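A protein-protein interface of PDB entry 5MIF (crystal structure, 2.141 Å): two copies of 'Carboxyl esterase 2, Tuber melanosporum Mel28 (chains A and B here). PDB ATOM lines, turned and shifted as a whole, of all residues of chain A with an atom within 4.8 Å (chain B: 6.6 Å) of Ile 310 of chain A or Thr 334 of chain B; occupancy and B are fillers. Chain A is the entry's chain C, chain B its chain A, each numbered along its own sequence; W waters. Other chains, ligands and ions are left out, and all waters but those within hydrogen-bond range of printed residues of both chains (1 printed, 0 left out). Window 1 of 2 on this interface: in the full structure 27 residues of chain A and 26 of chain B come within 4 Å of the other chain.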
ATOM      1  N   LEU A 280       9.010  19.912 -12.364  1.00  0.00           N
ATOM      2  CA  LEU A 280       8.746  19.545 -10.972  1.00  0.00           C
ATOM      3  C   LEU A 280       7.348  18.954 -10.914  1.00  0.00           C
ATOM      4  O   LEU A 280       6.383  19.576 -11.391  1.00  0.00           O
ATOM      5  CB  LEU A 280       8.853  20.761 -10.042  1.00  0.00           C
ATOM      6  CG  LEU A 280       8.274  20.638  -8.622  1.00  0.00           C
ATOM      7  CD1 LEU A 280       9.079  19.661  -7.761  1.00  0.00           C
ATOM      8  CD2 LEU A 280       8.161  21.989  -7.938  1.00  0.00           C
ATOM      9  N   ILE A 281       7.230  17.746 -10.377  1.00  0.00           N
ATOM     10  CA  ILE A 281       5.928  17.122 -10.209  1.00  0.00           C
ATOM     11  C   ILE A 281       5.648  17.036  -8.710  1.00  0.00           C
ATOM     12  O   ILE A 281       6.513  16.633  -7.933  1.00  0.00           O
ATOM     13  CB  ILE A 281       5.861  15.731 -10.853  1.00  0.00           C
ATOM     14  CG1 ILE A 281       6.144  15.827 -12.342  1.00  0.00           C
ATOM     15  CG2 ILE A 281       4.488  15.073 -10.627  1.00  0.00           C
ATOM     16  CD1 ILE A 281       6.262  14.483 -13.024  1.00  0.00           C
ATOM     17  N   VAL A 282       4.467  17.499  -8.306  1.00  0.00           N
ATOM     18  CA  VAL A 282       4.024  17.438  -6.918  1.00  0.00           C
ATOM     19  C   VAL A 282       2.757  16.586  -6.883  1.00  0.00           C
ATOM     20  O   VAL A 282       1.837  16.758  -7.683  1.00  0.00           O
ATOM     21  CB  VAL A 282       3.787  18.835  -6.327  1.00  0.00           C
ATOM     22  CG1 VAL A 282       3.221  18.745  -4.928  1.00  0.00           C
ATOM     23  CG2 VAL A 282       5.092  19.617  -6.324  1.00  0.00           C
ATOM     24  N   VAL A 283       2.735  15.638  -5.966  1.00  0.00           N
ATOM     25  CA  VAL A 283       1.655  14.683  -5.899  1.00  0.00           C
ATOM     26  C   VAL A 283       1.061  14.578  -4.491  1.00  0.00           C
ATOM     27  O   VAL A 283       1.767  14.777  -3.505  1.00  0.00           O
ATOM     28  CB  VAL A 283       2.240  13.353  -6.431  1.00  0.00           C
ATOM     29  CG1 VAL A 283       2.277  12.263  -5.391  1.00  0.00           C
ATOM     30  CG2 VAL A 283       1.616  12.962  -7.771  1.00  0.00           C
ATOM     31  N   ALA A 308      12.064  16.596 -10.881  1.00  0.00           N
ATOM     32  CA  ALA A 308      11.875  16.401  -9.438  1.00  0.00           C
ATOM     33  C   ALA A 308      10.458  15.876  -9.120  1.00  0.00           C
ATOM     34  O   ALA A 308       9.462  16.345  -9.696  1.00  0.00           O
ATOM     35  CB  ALA A 308      12.140  17.709  -8.700  1.00  0.00           C
ATOM     36  N   ILE A 309      10.355  14.896  -8.225  1.00  0.00           N
ATOM     37  CA  ILE A 309       9.043  14.373  -7.841  1.00  0.00           C
ATOM     38  C   ILE A 309       8.877  14.335  -6.337  1.00  0.00           C
ATOM     39  O   ILE A 309       9.653  13.681  -5.638  1.00  0.00           O
ATOM     40  CB  ILE A 309       8.808  12.969  -8.366  1.00  0.00           C
ATOM     41  CG1 ILE A 309       9.330  12.828  -9.799  1.00  0.00           C
ATOM     42  CG2 ILE A 309       7.346  12.618  -8.269  1.00  0.00           C
ATOM     43  CD1 ILE A 309       9.803  11.433 -10.115  1.00  0.00           C
ATOM     44  N   ILE A 310       7.829  14.987  -5.847  1.00  0.00           N
ATOM     45  CA  ILE A 310       7.615  15.115  -4.418  1.00  0.00           C
ATOM     46  C   ILE A 310       6.208  14.656  -4.033  1.00  0.00           C
ATOM     47  O   ILE A 310       5.222  15.069  -4.639  1.00  0.00           O
ATOM     48  CB  ILE A 310       7.847  16.571  -3.994  1.00  0.00           C
ATOM     49  CG1 ILE A 310       9.346  16.856  -3.920  1.00  0.00           C
ATOM     50  CG2 ILE A 310       7.194  16.875  -2.690  1.00  0.00           C
ATOM     51  CD1 ILE A 310       9.633  18.323  -3.869  1.00  0.00           C
ATOM     52  N   ARG A 311       6.127  13.786  -3.033  1.00  0.00           N
ATOM     53  CA  ARG A 311       4.857  13.291  -2.514  1.00  0.00           C
ATOM     54  C   ARG A 311       4.557  13.954  -1.177  1.00  0.00           C
ATOM     55  O   ARG A 311       5.390  13.907  -0.261  1.00  0.00           O
ATOM     56  CB  ARG A 311       4.894  11.764  -2.352  1.00  0.00           C
ATOM     57  CG  ARG A 311       3.656  11.203  -1.665  1.00  0.00           C
ATOM     58  CD  ARG A 311       3.815   9.755  -1.208  1.00  0.00           C
ATOM     59  NE  ARG A 311       4.047   8.851  -2.328  1.00  0.00           N
ATOM     60  CZ  ARG A 311       3.961   7.527  -2.245  1.00  0.00           C
ATOM     61  NH1 ARG A 311       3.627   6.953  -1.096  1.00  0.00           N
ATOM     62  NH2 ARG A 311       4.177   6.779  -3.314  1.00  0.00           N
ATOM     63  N   VAL A 312       3.383  14.585  -1.078  1.00  0.00           N
ATOM     64  CA  VAL A 312       2.955  15.267   0.144  1.00  0.00           C
ATOM     65  C   VAL A 312       2.041  14.361   0.965  1.00  0.00           C
ATOM     66  O   VAL A 312       0.986  13.939   0.491  1.00  0.00           O
ATOM     67  CB  VAL A 312       2.221  16.586  -0.169  1.00  0.00           C
ATOM     68  CG1 VAL A 312       1.973  17.365   1.111  1.00  0.00           C
ATOM     69  CG2 VAL A 312       3.031  17.411  -1.160  1.00  0.00           C
ATOM     70  N   LEU A 337       6.670  26.208  -2.317  1.00  0.00           N
ATOM     71  CA  LEU A 337       7.748  25.587  -3.073  1.00  0.00           C
ATOM     72  C   LEU A 337       7.586  25.839  -4.564  1.00  0.00           C
ATOM     73  O   LEU A 337       8.501  26.330  -5.222  1.00  0.00           O
ATOM     74  CB  LEU A 337       7.814  24.081  -2.829  1.00  0.00           C
ATOM     75  CG  LEU A 337       8.896  23.423  -3.702  1.00  0.00           C
ATOM     76  CD1 LEU A 337      10.294  23.955  -3.352  1.00  0.00           C
ATOM     77  CD2 LEU A 337       8.856  21.901  -3.622  1.00  0.00           C
ATOM     78  N   LEU B 280       8.536  20.635   9.917  1.00  0.00           N
ATOM     79  CA  LEU B 280       8.581  20.132   8.549  1.00  0.00           C
ATOM     80  C   LEU B 280       9.511  18.914   8.479  1.00  0.00           C
ATOM     81  O   LEU B 280      10.685  18.992   8.865  1.00  0.00           O
ATOM     82  CB  LEU B 280       9.059  21.226   7.586  1.00  0.00           C
ATOM     83  CG  LEU B 280       9.492  20.762   6.192  1.00  0.00           C
ATOM     84  CD1 LEU B 280       8.311  20.216   5.383  1.00  0.00           C
ATOM     85  CD2 LEU B 280      10.152  21.895   5.447  1.00  0.00           C
ATOM     86  N   VAL B 282      11.229  16.073   5.945  1.00  0.00           N
ATOM     87  CA  VAL B 282      11.555  15.709   4.576  1.00  0.00           C
ATOM     88  C   VAL B 282      12.264  14.357   4.602  1.00  0.00           C
ATOM     89  O   VAL B 282      13.198  14.175   5.373  1.00  0.00           O
ATOM     90  CB  VAL B 282      12.445  16.789   3.920  1.00  0.00           C
ATOM     91  CG1 VAL B 282      12.824  16.389   2.521  1.00  0.00           C
ATOM     92  CG2 VAL B 282      11.716  18.135   3.915  1.00  0.00           C
ATOM     93  N   ILE B 310       7.050  15.497   3.619  1.00  0.00           N
ATOM     94  CA  ILE B 310       7.342  15.412   2.203  1.00  0.00           C
ATOM     95  C   ILE B 310       8.347  14.307   1.889  1.00  0.00           C
ATOM     96  O   ILE B 310       9.412  14.226   2.502  1.00  0.00           O
ATOM     97  CB  ILE B 310       7.876  16.751   1.703  1.00  0.00           C
ATOM     98  CG1 ILE B 310       6.710  17.700   1.428  1.00  0.00           C
ATOM     99  CG2 ILE B 310       8.686  16.587   0.449  1.00  0.00           C
ATOM    100  CD1 ILE B 310       7.179  19.121   1.269  1.00  0.00           C
ATOM    101  N   ARG B 311       7.990  13.461   0.932  1.00  0.00           N
ATOM    102  CA  ARG B 311       8.853  12.396   0.447  1.00  0.00           C
ATOM    103  C   ARG B 311       9.400  12.768  -0.918  1.00  0.00           C
ATOM    104  O   ARG B 311       8.640  13.067  -1.843  1.00  0.00           O
ATOM    105  CB  ARG B 311       8.096  11.062   0.360  1.00  0.00           C
ATOM    106  CG  ARG B 311       8.911   9.941  -0.317  1.00  0.00           C
ATOM    107  CD  ARG B 311       8.044   8.734  -0.697  1.00  0.00           C
ATOM    108  NE  ARG B 311       7.449   8.073   0.462  1.00  0.00           N
ATOM    109  CZ  ARG B 311       6.838   6.888   0.418  1.00  0.00           C
ATOM    110  NH1 ARG B 311       6.724   6.234  -0.736  1.00  0.00           N
ATOM    111  NH2 ARG B 311       6.328   6.363   1.528  1.00  0.00           N
ATOM    112  N   VAL B 312      10.722  12.745  -1.042  1.00  0.00           N
ATOM    113  CA  VAL B 312      11.390  13.091  -2.281  1.00  0.00           C
ATOM    114  C   VAL B 312      11.702  11.816  -3.033  1.00  0.00           C
ATOM    115  O   VAL B 312      12.438  10.964  -2.534  1.00  0.00           O
ATOM    116  CB  VAL B 312      12.697  13.876  -2.017  1.00  0.00           C
ATOM    117  CG1 VAL B 312      13.252  14.430  -3.309  1.00  0.00           C
ATOM    118  CG2 VAL B 312      12.446  14.991  -1.030  1.00  0.00           C
ATOM    119  N   LEU B 313      11.145  11.668  -4.227  1.00  0.00           N
ATOM    120  CA  LEU B 313      11.321  10.419  -4.965  1.00  0.00           C
ATOM    121  C   LEU B 313      12.670  10.361  -5.685  1.00  0.00           C
ATOM    122  O   LEU B 313      13.233  11.394  -6.057  1.00  0.00           O
ATOM    123  CB  LEU B 313      10.182  10.215  -5.964  1.00  0.00           C
ATOM    124  CG  LEU B 313       8.948   9.515  -5.398  1.00  0.00           C
ATOM    125  CD1 LEU B 313       8.264  10.371  -4.310  1.00  0.00           C
ATOM    126  CD2 LEU B 313       7.977   9.157  -6.511  1.00  0.00           C
ATOM    127  N   PHE B 319      20.968  13.084   1.123  1.00  0.00           N
ATOM    128  CA  PHE B 319      20.933  13.989  -0.034  1.00  0.00           C
ATOM    129  C   PHE B 319      21.096  15.461   0.338  1.00  0.00           C
ATOM    130  O   PHE B 319      21.522  16.263  -0.488  1.00  0.00           O
ATOM    131  CB  PHE B 319      19.648  13.799  -0.871  1.00  0.00           C
ATOM    132  CG  PHE B 319      18.359  14.251  -0.202  1.00  0.00           C
ATOM    133  CD1 PHE B 319      18.045  15.603  -0.067  1.00  0.00           C
ATOM    134  CD2 PHE B 319      17.415  13.315   0.189  1.00  0.00           C
ATOM    135  CE1 PHE B 319      16.852  15.999   0.514  1.00  0.00           C
ATOM    136  CE2 PHE B 319      16.208  13.701   0.762  1.00  0.00           C
ATOM    137  CZ  PHE B 319      15.925  15.042   0.930  1.00  0.00           C
ATOM    138  N   ALA B 320      20.787  15.817   1.578  1.00  0.00           N
ATOM    139  CA  ALA B 320      20.839  17.213   1.987  1.00  0.00           C
ATOM    140  C   ALA B 320      22.249  17.704   2.334  1.00  0.00           C
ATOM    141  O   ALA B 320      22.486  18.908   2.339  1.00  0.00           O
ATOM    142  CB  ALA B 320      19.898  17.447   3.172  1.00  0.00           C
ATOM    143  N   PRO B 329      17.668  17.362  -8.918  1.00  0.00           N
ATOM    144  CA  PRO B 329      16.486  18.244  -8.906  1.00  0.00           C
ATOM    145  C   PRO B 329      15.676  18.180  -7.612  1.00  0.00           C
ATOM    146  O   PRO B 329      15.461  19.220  -6.995  1.00  0.00           O
ATOM    147  CB  PRO B 329      15.649  17.726 -10.079  1.00  0.00           C
ATOM    148  CG  PRO B 329      16.631  17.098 -11.000  1.00  0.00           C
ATOM    149  CD  PRO B 329      17.745  16.552 -10.149  1.00  0.00           C
ATOM    150  N   GLY B 330      15.255  16.984  -7.206  1.00  0.00           N
ATOM    151  CA  GLY B 330      14.459  16.819  -6.001  1.00  0.00           C
ATOM    152  C   GLY B 330      15.155  17.289  -4.740  1.00  0.00           C
ATOM    153  O   GLY B 330      14.571  17.994  -3.916  1.00  0.00           O
ATOM    154  N   ALA B 331      16.411  16.897  -4.586  1.00  0.00           N
ATOM    155  CA  ALA B 331      17.218  17.321  -3.447  1.00  0.00           C
ATOM    156  C   ALA B 331      17.390  18.844  -3.430  1.00  0.00           C
ATOM    157  O   ALA B 331      17.193  19.498  -2.411  1.00  0.00           O
ATOM    158  CB  ALA B 331      18.574  16.638  -3.480  1.00  0.00           C
ATOM    159  N   LYS B 332      17.774  19.398  -4.572  1.00  0.00           N
ATOM    160  CA  LYS B 332      18.007  20.826  -4.675  1.00  0.00           C
ATOM    161  C   LYS B 332      16.742  21.592  -4.314  1.00  0.00           C
ATOM    162  O   LYS B 332      16.794  22.569  -3.582  1.00  0.00           O
ATOM    163  CB  LYS B 332      18.465  21.186  -6.090  1.00  0.00           C
ATOM    164  CG  LYS B 332      18.931  22.626  -6.274  1.00  0.00           C
ATOM    165  CD  LYS B 332      19.255  22.891  -7.744  1.00  0.00           C
ATOM    166  CE  LYS B 332      20.542  23.680  -7.916  1.00  0.00           C
ATOM    167  NZ  LYS B 332      20.506  24.967  -7.155  1.00  0.00           N
ATOM    168  N   ALA B 333      15.601  21.121  -4.810  1.00  0.00           N
ATOM    169  CA  ALA B 333      14.339  21.813  -4.587  1.00  0.00           C
ATOM    170  C   ALA B 333      13.973  21.803  -3.107  1.00  0.00           C
ATOM    171  O   ALA B 333      13.509  22.808  -2.559  1.00  0.00           O
ATOM    172  CB  ALA B 333      13.224  21.182  -5.420  1.00  0.00           C
ATOM    173  N   THR B 334      14.196  20.673  -2.450  1.00  0.00           N
ATOM    174  CA  THR B 334      13.765  20.574  -1.066  1.00  0.00           C
ATOM    175  C   THR B 334      14.729  21.299  -0.136  1.00  0.00           C
ATOM    176  O   THR B 334      14.319  21.835   0.893  1.00  0.00           O
ATOM    177  CB  THR B 334      13.593  19.112  -0.642  1.00  0.00           C
ATOM    178  OG1 THR B 334      14.839  18.444  -0.753  1.00  0.00           O
ATOM    179  CG2 THR B 334      12.601  18.430  -1.576  1.00  0.00           C
ATOM    180  N   ILE B 335      16.001  21.372  -0.518  1.00  0.00           N
ATOM    181  CA  ILE B 335      16.959  22.133   0.276  1.00  0.00           C
ATOM    182  C   ILE B 335      16.605  23.621   0.271  1.00  0.00           C
ATOM    183  O   ILE B 335      16.635  24.271   1.315  1.00  0.00           O
ATOM    184  CB  ILE B 335      18.407  21.916  -0.222  1.00  0.00           C
ATOM    185  CG1 ILE B 335      18.861  20.488   0.131  1.00  0.00           C
ATOM    186  CG2 ILE B 335      19.363  22.910   0.430  1.00  0.00           C
ATOM    187  CD1 ILE B 335      20.127  20.043  -0.581  1.00  0.00           C
ATOM    188  N   GLU B 336      16.235  24.172  -0.878  1.00  0.00           N
ATOM    189  CA  GLU B 336      15.848  25.579  -0.859  1.00  0.00           C
ATOM    190  C   GLU B 336      14.482  25.774  -0.190  1.00  0.00           C
ATOM    191  O   GLU B 336      14.272  26.785   0.466  1.00  0.00           O
ATOM    192  CB  GLU B 336      15.880  26.184  -2.268  1.00  0.00           C
ATOM    193  CG  GLU B 336      15.377  25.302  -3.361  1.00  0.00           C
ATOM    194  CD  GLU B 336      16.043  25.602  -4.706  1.00  0.00           C
ATOM    195  OE1 GLU B 336      17.114  26.255  -4.728  1.00  0.00           O
ATOM    196  OE2 GLU B 336      15.501  25.166  -5.741  1.00  0.00           O
ATOM    197  N   LEU B 337      13.579  24.802  -0.314  1.00  0.00           N
ATOM    198  CA  LEU B 337      12.310  24.848   0.422  1.00  0.00           C
ATOM    199  C   LEU B 337      12.583  24.987   1.922  1.00  0.00           C
ATOM    200  O   LEU B 337      12.007  25.849   2.608  1.00  0.00           O
ATOM    201  CB  LEU B 337      11.465  23.592   0.161  1.00  0.00           C
ATOM    202  CG  LEU B 337      10.142  23.516   0.942  1.00  0.00           C
ATOM    203  CD1 LEU B 337       9.195  24.632   0.527  1.00  0.00           C
ATOM    204  CD2 LEU B 337       9.468  22.161   0.794  1.00  0.00           C
ATOM    205  N   ILE B 338      13.483  24.143   2.425  1.00  0.00           N
ATOM    206  CA  ILE B 338      13.847  24.180   3.837  1.00  0.00           C
ATOM    207  C   ILE B 338      14.323  25.566   4.254  1.00  0.00           C
ATOM    208  O   ILE B 338      13.792  26.140   5.213  1.00  0.00           O
ATOM    209  CB  ILE B 338      14.935  23.128   4.171  1.00  0.00           C
ATOM    210  CG1 ILE B 338      14.305  21.738   4.245  1.00  0.00           C
ATOM    211  CG2 ILE B 338      15.586  23.442   5.499  1.00  0.00           C
ATOM    212  CD1 ILE B 338      15.305  20.589   4.164  1.00  0.00           C
ATOM    213  N   GLY B 339      15.288  26.121   3.519  1.00  0.00           N
ATOM    214  CA  GLY B 339      15.784  27.456   3.816  1.00  0.00           C
ATOM    215  C   GLY B 339      14.687  28.497   3.671  1.00  0.00           C
ATOM    216  O   GLY B 339      14.536  29.391   4.514  1.00  0.00           O
HETATM  217  O   HOH W   1      12.693  13.960  -7.120  1.00  0.00           O
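The backbone carbonyl oxygen (O) of Arg 311 of chain B lies within hydrogen-bond range of the backbone NH (N) of Arg 311 of chain A, at 2.9 Å.
The backbone carbonyl oxygen (O) of Ile 309 of chain A sits at hydrogen-bond distance from the backbone NH (N) of Leu 313 of chain B.
The side-chain hydroxyl (OG1) of Thr 334 of chain B lies close to the backbone carbonyl oxygen (O) of Gly 330 of chain B (3.2 Å).
O of Ala 331 of chain B lies within hydrogen-bond range of OG1 of Thr 334 of chain B (3.1 Å).
O of Ala 308 of chain A sits at hydrogen-bond distance from N of Ile 281 of chain A (2.7 Å).
The backbone carbonyl oxygen of Ile 281 of chain A sits at hydrogen-bond distance from the backbone NH of Ile 310 of chain A, 3.0 Å away.
N of Val 283 of chain A is in hydrogen-bond range of O of Ile 310 of chain A (2.9 Å).
Ile 310 of chain A touches its own counterpart, Ile 310 of chain B.
Ile 310 of chain A touches Arg 311 of chain B, and with the chains exchanged Arg 311 of chain A touches Ile 310 of chain B.
Arg 311 of chain A touches its own counterpart, Arg 311 of chain B.
Leu 337 of chain B touches its own counterpart, Leu 337 of chain A.
Positions printed for both chains: 280, 282, 310, 311, 312 and 337.
Of the 12 pairs that touch across the chains among the printed residues, 5 have their exchanged pair printed and touching as well.
Among the printed residues, merely in contact across the chains: Ile 310 of chain A with Arg 311 of chain B, Arg 311 of chain A with Ile 310 of chain B, Ile 310 of chain A with Ile 310 of chain B, Leu 337 of chain A with Ala 333 of chain B, Ala 308 of chain A with Gly 330 of chain B, Leu 337 of chain A with Leu 337 of chain B, Ala 308 of chain A with Pro 329 of chain B, Ile 310 of chain A with Thr 334 of chain B, Ile 309 of chain A with Val 312 of chain B and Ile 309 of chain A with Arg 311 of chain B.
Of chain B, only Ile 310 (3.5 Å), Arg 311 (3.4 Å) and Thr 334 (3.8 Å) come within 4 Å of Ile 310 of chain A.
Of the printed residues of chain A, Thr 334 of chain B touches Ile 310.
Of the printed residues of chain B, Leu 337 of chain A touches Ala 333 (3.5 Å) and Leu 337 (3.7 Å).
Printed residues of chain A within 4 Å of Ala 333 of chain B: Leu 337.
Of the printed residues of chain A, Leu 337 of chain B touches Leu 337.
Leu 280 of chain B touches none of the printed residues of chain A.
Val 283 of chain A touches none of the printed residues of chain B.
The nearest residue of chain B that does not touch Ile 310 of chain A is Val 312 of chain B (4.6 Å).
The nearest printed residue of chain A that does not touch Thr 334 of chain B is Leu 337 of chain A (5.2 Å).
The nearest printed residue of chain A that does not touch Pro 329 of chain B is Ile 309 of chain A (6.3 Å).
Hydrophobic or aromatic side chains of chain A that line the printed part of chain B: Ala 308, Ile 309, Ile 310 and Leu 337.
Of the 19 printed residues of chain B, 9 touch a printed residue of chain A.
Water W1 bridges the backbone NH (N) of Ile 309 of chain A (2.8 Å) and the backbone carbonyl oxygen (O) of Leu 313 of chain B (2.8 Å).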
